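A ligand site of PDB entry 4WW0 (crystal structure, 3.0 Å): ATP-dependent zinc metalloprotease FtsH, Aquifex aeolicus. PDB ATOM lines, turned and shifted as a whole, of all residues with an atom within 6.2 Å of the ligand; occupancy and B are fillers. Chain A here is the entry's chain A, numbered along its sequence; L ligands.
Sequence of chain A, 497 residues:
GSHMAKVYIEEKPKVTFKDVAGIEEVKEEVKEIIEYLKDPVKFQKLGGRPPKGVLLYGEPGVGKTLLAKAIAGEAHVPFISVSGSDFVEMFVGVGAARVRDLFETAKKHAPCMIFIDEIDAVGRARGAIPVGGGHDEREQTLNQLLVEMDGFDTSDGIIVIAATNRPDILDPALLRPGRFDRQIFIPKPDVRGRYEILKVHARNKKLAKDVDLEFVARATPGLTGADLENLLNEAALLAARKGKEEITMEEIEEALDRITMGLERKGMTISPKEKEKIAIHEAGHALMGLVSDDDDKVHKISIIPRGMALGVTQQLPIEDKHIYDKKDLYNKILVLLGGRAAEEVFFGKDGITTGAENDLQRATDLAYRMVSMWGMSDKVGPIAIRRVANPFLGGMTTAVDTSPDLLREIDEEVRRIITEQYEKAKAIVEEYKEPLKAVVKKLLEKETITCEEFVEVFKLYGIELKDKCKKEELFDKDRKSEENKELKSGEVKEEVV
A ring nitrogen (NE2) of His 201 is in hydrogen-bond range of a nitrogen (N5) of the ligand, at 2.9 Å.
The side-chain carboxylate (OE2) of Glu 229 sits at hydrogen-bond distance from an oxygen (O9) of the ligand.
O5 of the ligand lies within hydrogen-bond range of N of Thr 65, at 3.0 Å.
An oxygen (O5) of the ligand sits at hydrogen-bond distance from the backbone NH (N) of Leu 66 (3.0 Å).
The side-chain amino group (NZ) of Lys 64 is in salt-bridge range of an oxygen (O3) of the ligand (2.8 Å).
The backbone NH of Val 62 is in hydrogen-bond range of an oxygen (O3) of the ligand (3.4 Å).
The backbone NH (N) of Gly 61 lies within hydrogen-bond range of an oxygen (O2) of the ligand (2.9 Å).
O of Ala 21 sits at hydrogen-bond distance from N3 of the ligand (2.9 Å).
An oxygen (O8) of the ligand lies close to the backbone NH of Ala 226 (3.4 Å).
An oxygen (O3) of the ligand is in hydrogen-bond range of the backbone NH (N) of Lys 64.
The side-chain hydroxyl (OG1) of Thr 65 lies within hydrogen-bond range of an oxygen (O5) of the ligand (2.9 Å).
The backbone NH of Ala 21 sits at hydrogen-bond distance from a nitrogen (N4) of the ligand.
The backbone NH (N) of Gly 63 is in hydrogen-bond range of an oxygen (O3) of the ligand, at 3.1 Å.
The backbone carbonyl oxygen of Gly 61 is in hydrogen-bond range of the backbone NH of Ala 226 (3.1 Å).
The side-chain amino group (NZ) of Lys 64 sits at hydrogen-bond distance from the backbone carbonyl oxygen (O) of Glu 59 (3.3 Å).
The side-chain amino group (NZ) of Lys 64 lies within hydrogen-bond range of the side-chain amide oxygen (OD1) of Asn 165, at 3.0 Å.
Asp 19 touches the ligand (O to C9, 3.3 Å).
C of Val 20 touches N4 of the ligand (3.9 Å).
Pro 60 touches the ligand (CA to O2, 3.8 Å).
Ile 197 touches the ligand.
CA of Gly 225 touches C6 of the ligand, at 3.6 Å.
15 residues have an atom within 4 Å of the ligand: Asp 19, Val 20, Ala 21, Pro 60, Gly 61, Val 62, Gly 63, Lys 64, Thr 65, Leu 66, Ile 197, His 201, Gly 225, Ala 226 and Glu 229.
The nearest printed residue that does not touch the ligand is Glu 59 (4.1 Å).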
ATOM      1  N   ASP A  19       4.409 -33.355   4.175  1.00  0.00           N
ATOM      2  CA  ASP A  19       3.918 -31.982   4.241  1.00  0.00           C
ATOM      3  C   ASP A  19       4.775 -31.082   3.321  1.00  0.00           C
ATOM      4  O   ASP A  19       4.440 -29.897   3.099  1.00  0.00           O
ATOM      5  CB  ASP A  19       3.916 -31.482   5.690  1.00  0.00           C
ATOM      6  CG  ASP A  19       3.260 -32.441   6.670  1.00  0.00           C
ATOM      7  OD1 ASP A  19       3.990 -33.140   7.399  1.00  0.00           O
ATOM      8  OD2 ASP A  19       2.020 -32.535   6.677  1.00  0.00           O
ATOM      9  N   VAL A  20       5.849 -31.649   2.767  1.00  0.00           N
ATOM     10  CA  VAL A  20       6.779 -30.968   1.858  1.00  0.00           C
ATOM     11  C   VAL A  20       6.527 -31.485   0.464  1.00  0.00           C
ATOM     12  O   VAL A  20       6.571 -32.690   0.255  1.00  0.00           O
ATOM     13  CB  VAL A  20       8.256 -31.170   2.280  1.00  0.00           C
ATOM     14  CG1 VAL A  20       9.203 -30.367   1.397  1.00  0.00           C
ATOM     15  CG2 VAL A  20       8.467 -30.798   3.744  1.00  0.00           C
ATOM     16  N   ALA A  21       6.371 -30.587  -0.501  1.00  0.00           N
ATOM     17  CA  ALA A  21       6.191 -31.005  -1.882  1.00  0.00           C
ATOM     18  C   ALA A  21       7.279 -30.438  -2.796  1.00  0.00           C
ATOM     19  O   ALA A  21       7.924 -29.431  -2.476  1.00  0.00           O
ATOM     20  CB  ALA A  21       4.821 -30.592  -2.386  1.00  0.00           C
ATOM     21  N   GLY A  22       7.476 -31.160  -3.897  1.00  0.00           N
ATOM     22  CA  GLY A  22       8.319 -30.839  -5.043  1.00  0.00           C
ATOM     23  C   GLY A  22       9.705 -30.244  -4.911  1.00  0.00           C
ATOM     24  O   GLY A  22       9.994 -29.216  -5.540  1.00  0.00           O
ATOM     25  N   ILE A  23      10.583 -30.913  -4.163  1.00  0.00           N
ATOM     26  CA  ILE A  23      12.008 -30.593  -3.982  1.00  0.00           C
ATOM     27  C   ILE A  23      12.704 -31.901  -3.638  1.00  0.00           C
ATOM     28  O   ILE A  23      13.522 -31.973  -2.705  1.00  0.00           O
ATOM     29  CB  ILE A  23      12.329 -29.453  -2.950  1.00  0.00           C
ATOM     30  CG1 ILE A  23      11.501 -29.532  -1.654  1.00  0.00           C
ATOM     31  CG2 ILE A  23      12.199 -28.104  -3.588  1.00  0.00           C
ATOM     32  CD1 ILE A  23      12.305 -29.263  -0.383  1.00  0.00           C
ATOM     33  N   GLY A  58      16.951 -19.138  -0.182  1.00  0.00           N
ATOM     34  CA  GLY A  58      15.966 -19.013  -1.230  1.00  0.00           C
ATOM     35  C   GLY A  58      15.063 -17.834  -0.991  1.00  0.00           C
ATOM     36  O   GLY A  58      15.209 -17.104  -0.002  1.00  0.00           O
ATOM     37  N   GLU A  59      14.102 -17.654  -1.887  1.00  0.00           N
ATOM     38  CA  GLU A  59      13.142 -16.562  -1.799  1.00  0.00           C
ATOM     39  C   GLU A  59      12.215 -16.746  -0.583  1.00  0.00           C
ATOM     40  O   GLU A  59      12.041 -17.866  -0.097  1.00  0.00           O
ATOM     41  CB  GLU A  59      12.317 -16.498  -3.101  1.00  0.00           C
ATOM     42  CG  GLU A  59      13.117 -16.093  -4.327  1.00  0.00           C
ATOM     43  CD  GLU A  59      12.969 -14.634  -4.702  1.00  0.00           C
ATOM     44  OE1 GLU A  59      13.737 -13.806  -4.165  1.00  0.00           O
ATOM     45  OE2 GLU A  59      12.064 -14.322  -5.513  1.00  0.00           O
ATOM     46  N   PRO A  60      11.606 -15.655  -0.067  1.00  0.00           N
ATOM     47  CA  PRO A  60      10.667 -15.839   1.056  1.00  0.00           C
ATOM     48  C   PRO A  60       9.460 -16.689   0.643  1.00  0.00           C
ATOM     49  O   PRO A  60       8.893 -16.470  -0.444  1.00  0.00           O
ATOM     50  CB  PRO A  60      10.254 -14.398   1.408  1.00  0.00           C
ATOM     51  CG  PRO A  60      11.295 -13.520   0.773  1.00  0.00           C
ATOM     52  CD  PRO A  60      11.703 -14.237  -0.464  1.00  0.00           C
ATOM     53  N   GLY A  61       9.175 -17.712   1.447  1.00  0.00           N
ATOM     54  CA  GLY A  61       8.044 -18.619   1.277  1.00  0.00           C
ATOM     55  C   GLY A  61       8.232 -19.877   0.475  1.00  0.00           C
ATOM     56  O   GLY A  61       7.256 -20.588   0.220  1.00  0.00           O
ATOM     57  N   VAL A  62       9.487 -20.196   0.091  1.00  0.00           N
ATOM     58  CA  VAL A  62       9.791 -21.393  -0.694  1.00  0.00           C
ATOM     59  C   VAL A  62       9.819 -22.693   0.197  1.00  0.00           C
ATOM     60  O   VAL A  62       9.895 -23.797  -0.373  1.00  0.00           O
ATOM     61  CB  VAL A  62      11.068 -21.281  -1.570  1.00  0.00           C
ATOM     62  CG1 VAL A  62      10.932 -20.171  -2.612  1.00  0.00           C
ATOM     63  CG2 VAL A  62      12.323 -21.091  -0.728  1.00  0.00           C
ATOM     64  N   GLY A  63       9.730 -22.557   1.522  1.00  0.00           N
ATOM     65  CA  GLY A  63       9.690 -23.681   2.450  1.00  0.00           C
ATOM     66  C   GLY A  63      10.973 -24.069   3.176  1.00  0.00           C
ATOM     67  O   GLY A  63      11.210 -25.260   3.462  1.00  0.00           O
ATOM     68  N   LYS A  64      11.783 -23.070   3.544  1.00  0.00           N
ATOM     69  CA  LYS A  64      13.050 -23.273   4.246  1.00  0.00           C
ATOM     70  C   LYS A  64      12.802 -23.716   5.677  1.00  0.00           C
ATOM     71  O   LYS A  64      13.385 -24.707   6.096  1.00  0.00           O
ATOM     72  CB  LYS A  64      13.911 -22.006   4.202  1.00  0.00           C
ATOM     73  CG  LYS A  64      14.394 -21.588   2.820  1.00  0.00           C
ATOM     74  CD  LYS A  64      15.015 -20.207   2.857  1.00  0.00           C
ATOM     75  CE  LYS A  64      14.177 -19.206   2.099  1.00  0.00           C
ATOM     76  NZ  LYS A  64      13.219 -18.431   2.940  1.00  0.00           N
ATOM     77  N   THR A  65      11.912 -23.020   6.430  1.00  0.00           N
ATOM     78  CA  THR A  65      11.614 -23.416   7.816  1.00  0.00           C
ATOM     79  C   THR A  65      10.862 -24.769   7.789  1.00  0.00           C
ATOM     80  O   THR A  65      11.139 -25.650   8.614  1.00  0.00           O
ATOM     81  CB  THR A  65      10.851 -22.349   8.640  1.00  0.00           C
ATOM     82  OG1 THR A  65       9.454 -22.346   8.313  1.00  0.00           O
ATOM     83  CG2 THR A  65      11.401 -20.942   8.464  1.00  0.00           C
ATOM     84  N   LEU A  66       9.979 -24.940   6.790  1.00  0.00           N
ATOM     85  CA  LEU A  66       9.213 -26.162   6.569  1.00  0.00           C
ATOM     86  C   LEU A  66      10.148 -27.365   6.374  1.00  0.00           C
ATOM     87  O   LEU A  66       9.953 -28.383   7.051  1.00  0.00           O
ATOM     88  CB  LEU A  66       8.305 -25.981   5.326  1.00  0.00           C
ATOM     89  CG  LEU A  66       7.526 -27.232   4.907  1.00  0.00           C
ATOM     90  CD1 LEU A  66       6.283 -27.437   5.770  1.00  0.00           C
ATOM     91  CD2 LEU A  66       7.168 -27.179   3.451  1.00  0.00           C
ATOM     92  N   LEU A  67      11.165 -27.237   5.484  1.00  0.00           N
ATOM     93  CA  LEU A  67      12.105 -28.318   5.221  1.00  0.00           C
ATOM     94  C   LEU A  67      12.859 -28.692   6.489  1.00  0.00           C
ATOM     95  O   LEU A  67      12.999 -29.885   6.778  1.00  0.00           O
ATOM     96  CB  LEU A  67      13.081 -27.962   4.103  1.00  0.00           C
ATOM     97  CG  LEU A  67      14.194 -28.995   3.865  1.00  0.00           C
ATOM     98  CD1 LEU A  67      13.640 -30.320   3.314  1.00  0.00           C
ATOM     99  CD2 LEU A  67      15.292 -28.406   3.017  1.00  0.00           C
ATOM    100  N   PHE A 115      17.512 -24.438  14.748  1.00  0.00           N
ATOM    101  CA  PHE A 115      17.071 -23.736  13.559  1.00  0.00           C
ATOM    102  C   PHE A 115      17.237 -22.223  13.755  1.00  0.00           C
ATOM    103  O   PHE A 115      16.644 -21.653  14.679  1.00  0.00           O
ATOM    104  CB  PHE A 115      15.631 -24.085  13.188  1.00  0.00           C
ATOM    105  CG  PHE A 115      15.193 -23.379  11.929  1.00  0.00           C
ATOM    106  CD1 PHE A 115      15.717 -23.738  10.688  1.00  0.00           C
ATOM    107  CD2 PHE A 115      14.334 -22.282  11.984  1.00  0.00           C
ATOM    108  CE1 PHE A 115      15.351 -23.053   9.531  1.00  0.00           C
ATOM    109  CE2 PHE A 115      13.987 -21.591  10.831  1.00  0.00           C
ATOM    110  CZ  PHE A 115      14.494 -21.978   9.614  1.00  0.00           C
ATOM    111  N   ASP A 117      16.508 -18.909  11.817  1.00  0.00           N
ATOM    112  CA  ASP A 117      15.859 -18.127  10.773  1.00  0.00           C
ATOM    113  C   ASP A 117      16.566 -16.774  10.701  1.00  0.00           C
ATOM    114  O   ASP A 117      17.049 -16.300  11.733  1.00  0.00           O
ATOM    115  CB  ASP A 117      14.384 -17.926  11.157  1.00  0.00           C
ATOM    116  CG  ASP A 117      13.389 -17.896  10.006  1.00  0.00           C
ATOM    117  OD1 ASP A 117      13.735 -18.386   8.903  1.00  0.00           O
ATOM    118  OD2 ASP A 117      12.237 -17.470  10.236  1.00  0.00           O
ATOM    119  N   ALA A 163      18.606 -20.387   7.929  1.00  0.00           N
ATOM    120  CA  ALA A 163      17.853 -19.974   6.748  1.00  0.00           C
ATOM    121  C   ALA A 163      18.027 -18.493   6.493  1.00  0.00           C
ATOM    122  O   ALA A 163      18.031 -17.705   7.453  1.00  0.00           O
ATOM    123  CB  ALA A 163      16.394 -20.310   6.906  1.00  0.00           C
ATOM    124  N   ASN A 165      17.162 -15.252   3.176  1.00  0.00           N
ATOM    125  CA  ASN A 165      16.583 -14.766   1.920  1.00  0.00           C
ATOM    126  C   ASN A 165      17.642 -13.952   1.201  1.00  0.00           C
ATOM    127  O   ASN A 165      17.568 -13.799  -0.021  1.00  0.00           O
ATOM    128  CB  ASN A 165      15.326 -13.922   2.175  1.00  0.00           C
ATOM    129  CG  ASN A 165      14.455 -14.400   3.299  1.00  0.00           C
ATOM    130  OD1 ASN A 165      13.798 -15.453   3.207  1.00  0.00           O
ATOM    131  ND2 ASN A 165      14.335 -13.597   4.361  1.00  0.00           N
ATOM    132  N   ILE A 197       2.178 -29.008  -4.259  1.00  0.00           N
ATOM    133  CA  ILE A 197       1.988 -28.116  -3.108  1.00  0.00           C
ATOM    134  C   ILE A 197       0.480 -27.867  -2.898  1.00  0.00           C
ATOM    135  O   ILE A 197      -0.010 -27.980  -1.771  1.00  0.00           O
ATOM    136  CB  ILE A 197       2.759 -26.779  -3.303  1.00  0.00           C
ATOM    137  CG1 ILE A 197       4.274 -27.013  -3.316  1.00  0.00           C
ATOM    138  CG2 ILE A 197       2.364 -25.731  -2.254  1.00  0.00           C
ATOM    139  CD1 ILE A 197       5.076 -25.843  -3.799  1.00  0.00           C
ATOM    140  N   VAL A 200      -1.195 -30.852  -1.276  1.00  0.00           N
ATOM    141  CA  VAL A 200      -0.814 -30.884   0.135  1.00  0.00           C
ATOM    142  C   VAL A 200      -1.693 -29.900   0.929  1.00  0.00           C
ATOM    143  O   VAL A 200      -2.278 -30.295   1.939  1.00  0.00           O
ATOM    144  CB  VAL A 200       0.715 -30.569   0.293  1.00  0.00           C
ATOM    145  CG1 VAL A 200       1.067 -30.017   1.667  1.00  0.00           C
ATOM    146  CG2 VAL A 200       1.569 -31.794  -0.041  1.00  0.00           C
ATOM    147  N   HIS A 201      -1.827 -28.665   0.442  1.00  0.00           N
ATOM    148  CA  HIS A 201      -2.582 -27.644   1.149  1.00  0.00           C
ATOM    149  C   HIS A 201      -4.093 -27.748   0.924  1.00  0.00           C
ATOM    150  O   HIS A 201      -4.849 -27.077   1.637  1.00  0.00           O
ATOM    151  CB  HIS A 201      -2.047 -26.255   0.816  1.00  0.00           C
ATOM    152  CG  HIS A 201      -0.688 -26.029   1.415  1.00  0.00           C
ATOM    153  ND1 HIS A 201      -0.479 -26.099   2.781  1.00  0.00           N
ATOM    154  CD2 HIS A 201       0.500 -25.791   0.811  1.00  0.00           C
ATOM    155  CE1 HIS A 201       0.814 -25.899   2.968  1.00  0.00           C
ATOM    156  NE2 HIS A 201       1.450 -25.692   1.815  1.00  0.00           N
ATOM    157  N   THR A 224       5.302 -18.974  -4.967  1.00  0.00           N
ATOM    158  CA  THR A 224       5.993 -19.833  -3.996  1.00  0.00           C
ATOM    159  C   THR A 224       4.960 -20.731  -3.321  1.00  0.00           C
ATOM    160  O   THR A 224       3.762 -20.487  -3.445  1.00  0.00           O
ATOM    161  CB  THR A 224       6.739 -18.982  -2.930  1.00  0.00           C
ATOM    162  OG1 THR A 224       5.794 -18.231  -2.161  1.00  0.00           O
ATOM    163  CG2 THR A 224       7.798 -18.078  -3.538  1.00  0.00           C
ATOM    164  N   GLY A 225       5.428 -21.744  -2.578  1.00  0.00           N
ATOM    165  CA  GLY A 225       4.554 -22.642  -1.835  1.00  0.00           C
ATOM    166  C   GLY A 225       3.650 -21.874  -0.884  1.00  0.00           C
ATOM    167  O   GLY A 225       2.471 -22.196  -0.746  1.00  0.00           O
ATOM    168  N   ALA A 226       4.202 -20.807  -0.268  1.00  0.00           N
ATOM    169  CA  ALA A 226       3.454 -19.929   0.641  1.00  0.00           C
ATOM    170  C   ALA A 226       2.315 -19.225  -0.099  1.00  0.00           C
ATOM    171  O   ALA A 226       1.190 -19.277   0.362  1.00  0.00           O
ATOM    172  CB  ALA A 226       4.386 -18.910   1.267  1.00  0.00           C
ATOM    173  N   ASP A 227       2.591 -18.613  -1.273  1.00  0.00           N
ATOM    174  CA  ASP A 227       1.582 -17.955  -2.096  1.00  0.00           C
ATOM    175  C   ASP A 227       0.428 -18.896  -2.407  1.00  0.00           C
ATOM    176  O   ASP A 227      -0.719 -18.485  -2.280  1.00  0.00           O
ATOM    177  CB  ASP A 227       2.189 -17.433  -3.416  1.00  0.00           C
ATOM    178  CG  ASP A 227       3.311 -16.434  -3.248  1.00  0.00           C
ATOM    179  OD1 ASP A 227       3.269 -15.641  -2.285  1.00  0.00           O
ATOM    180  OD2 ASP A 227       4.218 -16.409  -4.117  1.00  0.00           O
ATOM    181  N   GLU A 229      -0.418 -21.723  -0.684  1.00  0.00           N
ATOM    182  CA  GLU A 229      -1.058 -22.053   0.587  1.00  0.00           C
ATOM    183  C   GLU A 229      -2.065 -20.936   0.955  1.00  0.00           C
ATOM    184  O   GLU A 229      -3.175 -21.236   1.392  1.00  0.00           O
ATOM    185  CB  GLU A 229       0.019 -22.222   1.678  1.00  0.00           C
ATOM    186  CG  GLU A 229      -0.535 -22.610   3.040  1.00  0.00           C
ATOM    187  CD  GLU A 229       0.382 -22.329   4.211  1.00  0.00           C
ATOM    188  OE1 GLU A 229       1.186 -21.377   4.124  1.00  0.00           O
ATOM    189  OE2 GLU A 229       0.262 -23.049   5.227  1.00  0.00           O
HETATM  190  P1  LIG L   1      10.398 -19.732   4.167  1.00  0.00           P
HETATM  191  O1  LIG L   1      10.928 -20.082   5.540  1.00  0.00           O
HETATM  192  O2  LIG L   1      10.430 -18.212   4.065  1.00  0.00           O
HETATM  193  O3  LIG L   1      11.191 -20.374   3.077  1.00  0.00           O
HETATM  194  P2  LIG L   1       8.179 -21.290   5.147  1.00  0.00           P
HETATM  195  O4  LIG L   1       7.876 -20.551   6.466  1.00  0.00           O
HETATM  196  O5  LIG L   1       9.130 -22.382   5.466  1.00  0.00           O
HETATM  197  O6  LIG L   1       8.885 -20.241   4.196  1.00  0.00           O
HETATM  198  O7  LIG L   1       6.802 -21.809   4.545  1.00  0.00           O
HETATM  199  C1  LIG L   1       5.655 -20.955   4.473  1.00  0.00           C
HETATM  200  C2  LIG L   1       4.411 -21.760   4.212  1.00  0.00           C
HETATM  201  O8  LIG L   1       4.379 -22.212   2.843  1.00  0.00           O
HETATM  202  C3  LIG L   1       4.190 -22.988   5.097  1.00  0.00           C
HETATM  203  O9  LIG L   1       2.898 -23.019   5.704  1.00  0.00           O
HETATM  204  C4  LIG L   1       4.467 -24.177   4.165  1.00  0.00           C
HETATM  205  O10 LIG L   1       3.636 -25.295   4.445  1.00  0.00           O
HETATM  206  C5  LIG L   1       4.181 -23.613   2.775  1.00  0.00           C
HETATM  207  N1  LIG L   1       5.074 -24.149   1.754  1.00  0.00           N
HETATM  208  C6  LIG L   1       6.181 -23.529   1.227  1.00  0.00           C
HETATM  209  N2  LIG L   1       6.880 -24.289   0.414  1.00  0.00           N
HETATM  210  C7  LIG L   1       6.190 -25.484   0.403  1.00  0.00           C
HETATM  211  C8  LIG L   1       6.432 -26.719  -0.233  1.00  0.00           C
HETATM  212  N3  LIG L   1       7.467 -26.948  -1.044  1.00  0.00           N
HETATM  213  N4  LIG L   1       5.573 -27.739   0.021  1.00  0.00           N
HETATM  214  C9  LIG L   1       4.531 -27.522   0.830  1.00  0.00           C
HETATM  215  N5  LIG L   1       4.194 -26.395   1.479  1.00  0.00           N
HETATM  216  C10 LIG L   1       5.066 -25.412   1.224  1.00  0.00           C
